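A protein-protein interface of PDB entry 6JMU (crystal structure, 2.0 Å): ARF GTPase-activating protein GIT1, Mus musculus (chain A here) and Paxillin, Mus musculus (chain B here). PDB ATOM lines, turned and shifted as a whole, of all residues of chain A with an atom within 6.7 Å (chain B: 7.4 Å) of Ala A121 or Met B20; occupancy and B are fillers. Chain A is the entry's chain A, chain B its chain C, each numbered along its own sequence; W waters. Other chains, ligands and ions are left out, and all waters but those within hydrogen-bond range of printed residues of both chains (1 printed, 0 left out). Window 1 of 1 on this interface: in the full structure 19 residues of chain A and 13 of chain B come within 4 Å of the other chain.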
ATOM      1  N   VAL A  28     -10.439  33.555 -31.819  1.00  0.00           N
ATOM      2  CA  VAL A  28     -10.099  33.262 -30.450  1.00  0.00           C
ATOM      3  C   VAL A  28      -8.748  32.567 -30.404  1.00  0.00           C
ATOM      4  O   VAL A  28      -7.886  32.946 -29.613  1.00  0.00           O
ATOM      5  CB  VAL A  28     -11.162  32.385 -29.781  1.00  0.00           C
ATOM      6  CG1 VAL A  28     -10.643  31.855 -28.473  1.00  0.00           C
ATOM      7  CG2 VAL A  28     -12.439  33.175 -29.584  1.00  0.00           C
ATOM      8  N   THR A  29      -8.558  31.566 -31.266  1.00  0.00           N
ATOM      9  CA  THR A  29      -7.351  30.739 -31.210  1.00  0.00           C
ATOM     10  C   THR A  29      -6.134  31.579 -31.537  1.00  0.00           C
ATOM     11  O   THR A  29      -5.076  31.389 -30.941  1.00  0.00           O
ATOM     12  CB  THR A  29      -7.420  29.511 -32.176  1.00  0.00           C
ATOM     13  OG1 THR A  29      -8.342  28.533 -31.672  1.00  0.00           O
ATOM     14  CG2 THR A  29      -6.054  28.840 -32.320  1.00  0.00           C
ATOM     15  N   ILE A  32      -5.243  33.822 -28.421  1.00  0.00           N
ATOM     16  CA  ILE A  32      -4.667  33.017 -27.336  1.00  0.00           C
ATOM     17  C   ILE A  32      -3.236  32.566 -27.665  1.00  0.00           C
ATOM     18  O   ILE A  32      -2.360  32.542 -26.786  1.00  0.00           O
ATOM     19  CB  ILE A  32      -5.542  31.774 -27.029  1.00  0.00           C
ATOM     20  CG1 ILE A  32      -6.881  32.197 -26.424  1.00  0.00           C
ATOM     21  CG2 ILE A  32      -4.818  30.795 -26.094  1.00  0.00           C
ATOM     22  CD1 ILE A  32      -7.835  31.027 -26.170  1.00  0.00           C
ATOM     23  N   LEU A  81     -17.060  29.103 -21.304  1.00  0.00           N
ATOM     24  CA  LEU A  81     -16.370  29.997 -22.231  1.00  0.00           C
ATOM     25  C   LEU A  81     -16.377  31.410 -21.683  1.00  0.00           C
ATOM     26  O   LEU A  81     -15.339  32.076 -21.617  1.00  0.00           O
ATOM     27  CB  LEU A  81     -17.021  29.976 -23.616  1.00  0.00           C
ATOM     28  CG  LEU A  81     -16.415  30.932 -24.643  1.00  0.00           C
ATOM     29  CD1 LEU A  81     -15.087  30.415 -25.186  1.00  0.00           C
ATOM     30  CD2 LEU A  81     -17.407  31.180 -25.753  1.00  0.00           C
ATOM     31  N   CYS A 116      -6.238  29.561 -17.510  1.00  0.00           N
ATOM     32  CA  CYS A 116      -7.465  30.198 -17.949  1.00  0.00           C
ATOM     33  C   CYS A 116      -7.606  30.144 -19.464  1.00  0.00           C
ATOM     34  O   CYS A 116      -8.704  29.941 -19.977  1.00  0.00           O
ATOM     35  CB  CYS A 116      -7.512  31.647 -17.475  1.00  0.00           C
ATOM     36  SG  CYS A 116      -7.815  31.824 -15.721  1.00  0.00           S
ATOM     37  N   ALA A 117      -6.499  30.328 -20.175  1.00  0.00           N
ATOM     38  CA  ALA A 117      -6.529  30.317 -21.626  1.00  0.00           C
ATOM     39  C   ALA A 117      -6.860  28.918 -22.124  1.00  0.00           C
ATOM     40  O   ALA A 117      -7.565  28.755 -23.113  1.00  0.00           O
ATOM     41  CB  ALA A 117      -5.205  30.798 -22.197  1.00  0.00           C
ATOM     42  N   TYR A 118      -6.347  27.910 -21.436  1.00  0.00           N
ATOM     43  CA  TYR A 118      -6.661  26.532 -21.783  1.00  0.00           C
ATOM     44  C   TYR A 118      -8.164  26.338 -21.741  1.00  0.00           C
ATOM     45  O   TYR A 118      -8.765  25.791 -22.668  1.00  0.00           O
ATOM     46  CB  TYR A 118      -5.972  25.556 -20.824  1.00  0.00           C
ATOM     47  CG  TYR A 118      -6.155  24.091 -21.163  1.00  0.00           C
ATOM     48  CD1 TYR A 118      -7.243  23.372 -20.683  1.00  0.00           C
ATOM     49  CD2 TYR A 118      -5.221  23.423 -21.932  1.00  0.00           C
ATOM     50  CE1 TYR A 118      -7.404  22.030 -20.982  1.00  0.00           C
ATOM     51  CE2 TYR A 118      -5.368  22.082 -22.236  1.00  0.00           C
ATOM     52  CZ  TYR A 118      -6.464  21.382 -21.763  1.00  0.00           C
ATOM     53  OH  TYR A 118      -6.613  20.038 -22.082  1.00  0.00           O
ATOM     54  N   ASP A 119      -8.761  26.806 -20.654  1.00  0.00           N
ATOM     55  CA  ASP A 119     -10.181  26.631 -20.430  1.00  0.00           C
ATOM     56  C   ASP A 119     -10.990  27.243 -21.561  1.00  0.00           C
ATOM     57  O   ASP A 119     -12.030  26.712 -21.937  1.00  0.00           O
ATOM     58  CB  ASP A 119     -10.606  27.255 -19.102  1.00  0.00           C
ATOM     59  CG  ASP A 119     -10.127  26.466 -17.894  1.00  0.00           C
ATOM     60  OD1 ASP A 119      -9.517  25.387 -18.066  1.00  0.00           O
ATOM     61  OD2 ASP A 119     -10.384  26.930 -16.767  1.00  0.00           O
ATOM     62  N   ILE A 120     -10.512  28.365 -22.088  1.00  0.00           N
ATOM     63  CA  ILE A 120     -11.207  29.037 -23.183  1.00  0.00           C
ATOM     64  C   ILE A 120     -11.175  28.175 -24.430  1.00  0.00           C
ATOM     65  O   ILE A 120     -12.206  27.914 -25.037  1.00  0.00           O
ATOM     66  CB  ILE A 120     -10.599  30.415 -23.497  1.00  0.00           C
ATOM     67  CG1 ILE A 120     -10.761  31.348 -22.296  1.00  0.00           C
ATOM     68  CG2 ILE A 120     -11.305  31.036 -24.702  1.00  0.00           C
ATOM     69  CD1 ILE A 120      -9.929  32.614 -22.376  1.00  0.00           C
ATOM     70  N   ALA A 121      -9.979  27.732 -24.794  1.00  0.00           N
ATOM     71  CA  ALA A 121      -9.782  26.848 -25.937  1.00  0.00           C
ATOM     72  C   ALA A 121     -10.634  25.580 -25.822  1.00  0.00           C
ATOM     73  O   ALA A 121     -11.244  25.139 -26.792  1.00  0.00           O
ATOM     74  CB  ALA A 121      -8.321  26.488 -26.065  1.00  0.00           C
ATOM     75  N   LYS A 122     -10.666  25.012 -24.620  1.00  0.00           N
ATOM     76  CA  LYS A 122     -11.470  23.834 -24.304  1.00  0.00           C
ATOM     77  C   LYS A 122     -12.953  24.087 -24.564  1.00  0.00           C
ATOM     78  O   LYS A 122     -13.608  23.328 -25.274  1.00  0.00           O
ATOM     79  CB  LYS A 122     -11.234  23.429 -22.839  1.00  0.00           C
ATOM     80  CG  LYS A 122     -12.007  22.218 -22.366  1.00  0.00           C
ATOM     81  CD  LYS A 122     -11.615  21.875 -20.943  1.00  0.00           C
ATOM     82  CE  LYS A 122     -12.319  20.623 -20.429  1.00  0.00           C
ATOM     83  NZ  LYS A 122     -13.784  20.823 -20.223  1.00  0.00           N
ATOM     84  N   ALA A 123     -13.470  25.167 -23.994  1.00  0.00           N
ATOM     85  CA  ALA A 123     -14.876  25.523 -24.152  1.00  0.00           C
ATOM     86  C   ALA A 123     -15.211  25.815 -25.607  1.00  0.00           C
ATOM     87  O   ALA A 123     -16.295  25.469 -26.081  1.00  0.00           O
ATOM     88  CB  ALA A 123     -15.212  26.709 -23.299  1.00  0.00           C
ATOM     89  N   ALA A 124     -14.281  26.453 -26.311  1.00  0.00           N
ATOM     90  CA  ALA A 124     -14.491  26.764 -27.711  1.00  0.00           C
ATOM     91  C   ALA A 124     -14.604  25.488 -28.544  1.00  0.00           C
ATOM     92  O   ALA A 124     -15.478  25.371 -29.388  1.00  0.00           O
ATOM     93  CB  ALA A 124     -13.382  27.629 -28.233  1.00  0.00           C
ATOM     94  N   LYS A 125     -13.707  24.540 -28.313  1.00  0.00           N
ATOM     95  CA  LYS A 125     -13.718  23.300 -29.062  1.00  0.00           C
ATOM     96  C   LYS A 125     -14.991  22.523 -28.769  1.00  0.00           C
ATOM     97  O   LYS A 125     -15.562  21.904 -29.654  1.00  0.00           O
ATOM     98  CB  LYS A 125     -12.462  22.488 -28.730  1.00  0.00           C
ATOM     99  CG  LYS A 125     -12.469  21.020 -29.142  1.00  0.00           C
ATOM    100  CD  LYS A 125     -11.420  20.280 -28.299  1.00  0.00           C
ATOM    101  CE  LYS A 125     -11.521  18.767 -28.400  1.00  0.00           C
ATOM    102  NZ  LYS A 125     -10.463  18.143 -27.551  1.00  0.00           N
ATOM    103  N   GLN A 126     -15.442  22.574 -27.524  1.00  0.00           N
ATOM    104  CA  GLN A 126     -16.700  21.945 -27.159  1.00  0.00           C
ATOM    105  C   GLN A 126     -17.811  22.474 -28.028  1.00  0.00           C
ATOM    106  O   GLN A 126     -18.633  21.731 -28.540  1.00  0.00           O
ATOM    107  CB  GLN A 126     -17.020  22.192 -25.686  1.00  0.00           C
ATOM    108  CG  GLN A 126     -16.353  21.203 -24.744  1.00  0.00           C
ATOM    109  CD  GLN A 126     -16.698  21.437 -23.289  1.00  0.00           C
ATOM    110  OE1 GLN A 126     -17.661  22.128 -22.967  1.00  0.00           O
ATOM    111  NE2 GLN A 126     -15.930  20.829 -22.401  1.00  0.00           N
ATOM    112  N   THR B  13     -11.329  22.058 -34.824  1.00  0.00           N
ATOM    113  CA  THR B  13     -10.995  21.331 -33.623  1.00  0.00           C
ATOM    114  C   THR B  13      -9.515  20.966 -33.598  1.00  0.00           C
ATOM    115  O   THR B  13      -8.868  21.089 -32.560  1.00  0.00           O
ATOM    116  CB  THR B  13     -11.873  20.091 -33.503  1.00  0.00           C
ATOM    117  OG1 THR B  13     -11.717  19.301 -34.684  1.00  0.00           O
ATOM    118  CG2 THR B  13     -13.325  20.513 -33.380  1.00  0.00           C
ATOM    119  N   ARG B  14      -8.972  20.549 -34.740  1.00  0.00           N
ATOM    120  CA  ARG B  14      -7.549  20.224 -34.807  1.00  0.00           C
ATOM    121  C   ARG B  14      -6.704  21.438 -34.450  1.00  0.00           C
ATOM    122  O   ARG B  14      -5.695  21.324 -33.769  1.00  0.00           O
ATOM    123  CB  ARG B  14      -7.152  19.708 -36.194  1.00  0.00           C
ATOM    124  CG  ARG B  14      -5.653  19.801 -36.502  1.00  0.00           C
ATOM    125  CD  ARG B  14      -5.098  18.464 -37.018  1.00  0.00           C
ATOM    126  NE  ARG B  14      -3.640  18.467 -37.171  1.00  0.00           N
ATOM    127  CZ  ARG B  14      -2.932  17.465 -37.694  1.00  0.00           C
ATOM    128  NH1 ARG B  14      -3.540  16.360 -38.116  1.00  0.00           N
ATOM    129  NH2 ARG B  14      -1.614  17.572 -37.798  1.00  0.00           N
ATOM    130  N   GLU B  15      -7.127  22.611 -34.893  1.00  0.00           N
ATOM    131  CA  GLU B  15      -6.398  23.821 -34.565  1.00  0.00           C
ATOM    132  C   GLU B  15      -6.566  24.169 -33.092  1.00  0.00           C
ATOM    133  O   GLU B  15      -5.688  24.779 -32.492  1.00  0.00           O
ATOM    134  CB  GLU B  15      -6.861  24.972 -35.438  1.00  0.00           C
ATOM    135  CG  GLU B  15      -6.055  26.233 -35.233  1.00  0.00           C
ATOM    136  CD  GLU B  15      -6.502  27.357 -36.139  1.00  0.00           C
ATOM    137  OE1 GLU B  15      -7.698  27.716 -36.093  1.00  0.00           O
ATOM    138  OE2 GLU B  15      -5.654  27.889 -36.887  1.00  0.00           O
ATOM    139  N   LEU B  16      -7.694  23.773 -32.512  1.00  0.00           N
ATOM    140  CA  LEU B  16      -7.935  23.982 -31.091  1.00  0.00           C
ATOM    141  C   LEU B  16      -7.121  23.004 -30.271  1.00  0.00           C
ATOM    142  O   LEU B  16      -6.538  23.366 -29.252  1.00  0.00           O
ATOM    143  CB  LEU B  16      -9.414  23.826 -30.779  1.00  0.00           C
ATOM    144  CG  LEU B  16     -10.197  25.074 -31.172  1.00  0.00           C
ATOM    145  CD1 LEU B  16     -11.626  24.731 -31.431  1.00  0.00           C
ATOM    146  CD2 LEU B  16     -10.099  26.127 -30.077  1.00  0.00           C
ATOM    147  N   ASP B  17      -7.084  21.758 -30.728  1.00  0.00           N
ATOM    148  CA  ASP B  17      -6.308  20.719 -30.058  1.00  0.00           C
ATOM    149  C   ASP B  17      -4.814  21.071 -30.107  1.00  0.00           C
ATOM    150  O   ASP B  17      -4.089  20.852 -29.148  1.00  0.00           O
ATOM    151  CB  ASP B  17      -6.566  19.339 -30.695  1.00  0.00           C
ATOM    152  CG  ASP B  17      -7.898  18.714 -30.266  1.00  0.00           C
ATOM    153  OD1 ASP B  17      -8.484  19.167 -29.273  1.00  0.00           O
ATOM    154  OD2 ASP B  17      -8.348  17.743 -30.910  1.00  0.00           O
ATOM    155  N   GLU B  18      -4.372  21.628 -31.227  1.00  0.00           N
ATOM    156  CA  GLU B  18      -3.000  22.113 -31.387  1.00  0.00           C
ATOM    157  C   GLU B  18      -2.659  23.168 -30.346  1.00  0.00           C
ATOM    158  O   GLU B  18      -1.573  23.177 -29.777  1.00  0.00           O
ATOM    159  CB  GLU B  18      -2.799  22.694 -32.793  1.00  0.00           C
ATOM    160  CG  GLU B  18      -2.274  21.706 -33.808  1.00  0.00           C
ATOM    161  CD  GLU B  18      -2.485  22.158 -35.237  1.00  0.00           C
ATOM    162  OE1 GLU B  18      -2.911  23.313 -35.452  1.00  0.00           O
ATOM    163  OE2 GLU B  18      -2.212  21.349 -36.149  1.00  0.00           O
ATOM    164  N   LEU B  19      -3.597  24.070 -30.109  1.00  0.00           N
ATOM    165  CA  LEU B  19      -3.374  25.150 -29.173  1.00  0.00           C
ATOM    166  C   LEU B  19      -3.405  24.641 -27.726  1.00  0.00           C
ATOM    167  O   LEU B  19      -2.584  25.043 -26.895  1.00  0.00           O
ATOM    168  CB  LEU B  19      -4.415  26.237 -29.397  1.00  0.00           C
ATOM    169  CG  LEU B  19      -4.355  27.322 -28.344  1.00  0.00           C
ATOM    170  CD1 LEU B  19      -3.004  28.005 -28.427  1.00  0.00           C
ATOM    171  CD2 LEU B  19      -5.491  28.288 -28.570  1.00  0.00           C
ATOM    172  N   MET B  20      -4.344  23.744 -27.436  1.00  0.00           N
ATOM    173  CA  MET B  20      -4.456  23.145 -26.114  1.00  0.00           C
ATOM    174  C   MET B  20      -3.214  22.327 -25.746  1.00  0.00           C
ATOM    175  O   MET B  20      -2.702  22.451 -24.639  1.00  0.00           O
ATOM    176  CB  MET B  20      -5.702  22.269 -26.034  1.00  0.00           C
ATOM    177  CG  MET B  20      -7.000  23.049 -26.121  1.00  0.00           C
ATOM    178  SD  MET B  20      -8.429  22.011 -26.490  1.00  0.00           S
ATOM    179  CE  MET B  20      -8.566  21.050 -24.989  1.00  0.00           C
ATOM    180  N   ALA B  21      -2.729  21.490 -26.661  1.00  0.00           N
ATOM    181  CA  ALA B  21      -1.466  20.796 -26.466  1.00  0.00           C
ATOM    182  C   ALA B  21      -0.321  21.755 -26.121  1.00  0.00           C
ATOM    183  O   ALA B  21       0.483  21.475 -25.252  1.00  0.00           O
ATOM    184  CB  ALA B  21      -1.121  20.004 -27.698  1.00  0.00           C
ATOM    185  N   SER B  22      -0.243  22.886 -26.807  1.00  0.00           N
ATOM    186  CA  SER B  22       0.832  23.847 -26.584  1.00  0.00           C
ATOM    187  C   SER B  22       0.730  24.508 -25.208  1.00  0.00           C
ATOM    188  O   SER B  22       1.727  24.656 -24.499  1.00  0.00           O
ATOM    189  CB  SER B  22       0.825  24.914 -27.683  1.00  0.00           C
ATOM    190  OG  SER B  22       1.104  24.351 -28.952  1.00  0.00           O
ATOM    191  N   LEU B  23      -0.485  24.906 -24.846  1.00  0.00           N
ATOM    192  CA  LEU B  23      -0.763  25.551 -23.566  1.00  0.00           C
ATOM    193  C   LEU B  23      -0.495  24.614 -22.384  1.00  0.00           C
ATOM    194  O   LEU B  23       0.108  25.020 -21.395  1.00  0.00           O
ATOM    195  CB  LEU B  23      -2.223  26.041 -23.515  1.00  0.00           C
ATOM    196  CG  LEU B  23      -2.725  27.216 -24.366  1.00  0.00           C
ATOM    197  CD1 LEU B  23      -4.238  27.331 -24.259  1.00  0.00           C
ATOM    198  CD2 LEU B  23      -2.055  28.548 -24.013  1.00  0.00           C
ATOM    199  N   SER B  24      -0.950  23.366 -22.476  1.00  0.00           N
ATOM    200  CA  SER B  24      -0.817  22.454 -21.352  1.00  0.00           C
ATOM    201  C   SER B  24       0.624  21.971 -21.238  1.00  0.00           C
ATOM    202  O   SER B  24       1.084  21.626 -20.158  1.00  0.00           O
ATOM    203  CB  SER B  24      -1.779  21.261 -21.476  1.00  0.00           C
ATOM    204  OG  SER B  24      -1.323  20.298 -22.406  1.00  0.00           O
ATOM    205  N   ASP B  25       1.337  21.954 -22.355  1.00  0.00           N
ATOM    206  CA  ASP B  25       2.743  21.585 -22.345  1.00  0.00           C
ATOM    207  C   ASP B  25       3.564  22.671 -21.651  1.00  0.00           C
ATOM    208  O   ASP B  25       4.499  22.373 -20.917  1.00  0.00           O
ATOM    209  CB  ASP B  25       3.234  21.355 -23.767  1.00  0.00           C
ATOM    210  CG  ASP B  25       4.530  20.625 -23.817  1.00  0.00           C
ATOM    211  OD1 ASP B  25       5.506  21.233 -24.291  1.00  0.00           O
ATOM    212  OD2 ASP B  25       4.574  19.452 -23.398  1.00  0.00           O
ATOM    213  N   PHE B  26       3.193  23.927 -21.889  1.00  0.00           N
ATOM    214  CA  PHE B  26       3.754  25.091 -21.192  1.00  0.00           C
ATOM    215  C   PHE B  26       3.545  24.955 -19.677  1.00  0.00           C
ATOM    216  O   PHE B  26       4.358  25.419 -18.870  1.00  0.00           O
ATOM    217  CB  PHE B  26       3.108  26.386 -21.716  1.00  0.00           C
ATOM    218  CG  PHE B  26       3.711  27.648 -21.149  1.00  0.00           C
ATOM    219  CD1 PHE B  26       4.762  28.290 -21.794  1.00  0.00           C
ATOM    220  CD2 PHE B  26       3.232  28.199 -19.968  1.00  0.00           C
ATOM    221  CE1 PHE B  26       5.320  29.464 -21.271  1.00  0.00           C
ATOM    222  CE2 PHE B  26       3.787  29.369 -19.442  1.00  0.00           C
ATOM    223  CZ  PHE B  26       4.833  30.000 -20.097  1.00  0.00           C
HETATM  224  O   HOH W   1     -10.384  16.318 -30.229  1.00  0.00           O
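The side-chain amino group (NZ) of Lys A125 lies within salt-bridge range of the side-chain carboxylate (OD1) of Asp B17 (2.8 Å).
Water W1 lies within hydrogen-bond range of the side-chain carboxylate (OD2) of Asp B17 (2.6 Å) and the side-chain amino group (NZ) of Lys A125 (3.2 Å).
The backbone carbonyl oxygen of Met B20 sits at hydrogen-bond distance from the side-chain hydroxyl of Ser B24, at 3.4 Å.
Among the printed residues, pairs that only touch across the chains: Thr A29 with Glu B15 (3.9 Å), Thr A29 with Leu B16 (3.4 Å), Thr A29 with Leu B19 (3.8 Å), Ile A32 with Leu B19 (3.6 Å), Ile A32 with Leu B23 (3.96 Å), Ala A117 with Leu B23 (3.7 Å), Tyr A118 with Met B20 (3.6 Å), Tyr A118 with Leu B23 (3.6 Å), Tyr A118 with Ser B24 (3.8 Å), Ala A121 with Leu B16 (3.6 Å), Ala A121 with Met B20 (3.7 Å), Lys A125 with Leu B16 (3.5 Å) and Lys A125 with Met B20 (3.9 Å).
Of the 15 printed residues of chain A, 6 touch a printed residue of chain B. Printed residues of chain A that touch a printed residue of chain B: Thr A29, Ile A32, Ala A117, Tyr A118, Ala A121 and Lys A125. Hydrophobic or aromatic side chains of chain A that line the printed part of chain B: Ile A32, Tyr A118 and Ala A121. Of the 14 printed residues of chain B, 7 touch a printed residue of chain A. Among the printed residues, 14 pairs touch across the chains. Among the printed residues, Asp or Glu carboxylates within 4 Å of a Lys or Arg side-chain nitrogen of the other chain: Lys A125 with Asp B17.
Of the printed residues of chain B, Ile A32 touches Leu B19 and Leu B23. Of chain B, only Leu B16 and Met B20 come within 4 Å of Ala A121. Arg B14 touches none of the printed residues of chain A. Of the printed residues of chain A, Leu B16 touches Thr A29, Ala A121 and Lys A125. Printed residues of chain A within 4 Å of Met B20: Tyr A118 (3.6 Å), Ala A121 (3.7 Å) and Lys A125 (3.9 Å). Of the printed residues of chain A, Leu B23 touches Ile A32, Ala A117 and Tyr A118. The nearest residue of chain B that does not touch Ala A121 is Leu B19 (4.2 Å). The nearest printed residue of chain B that does not touch Ala A117 is Leu B19 (5.9 Å).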
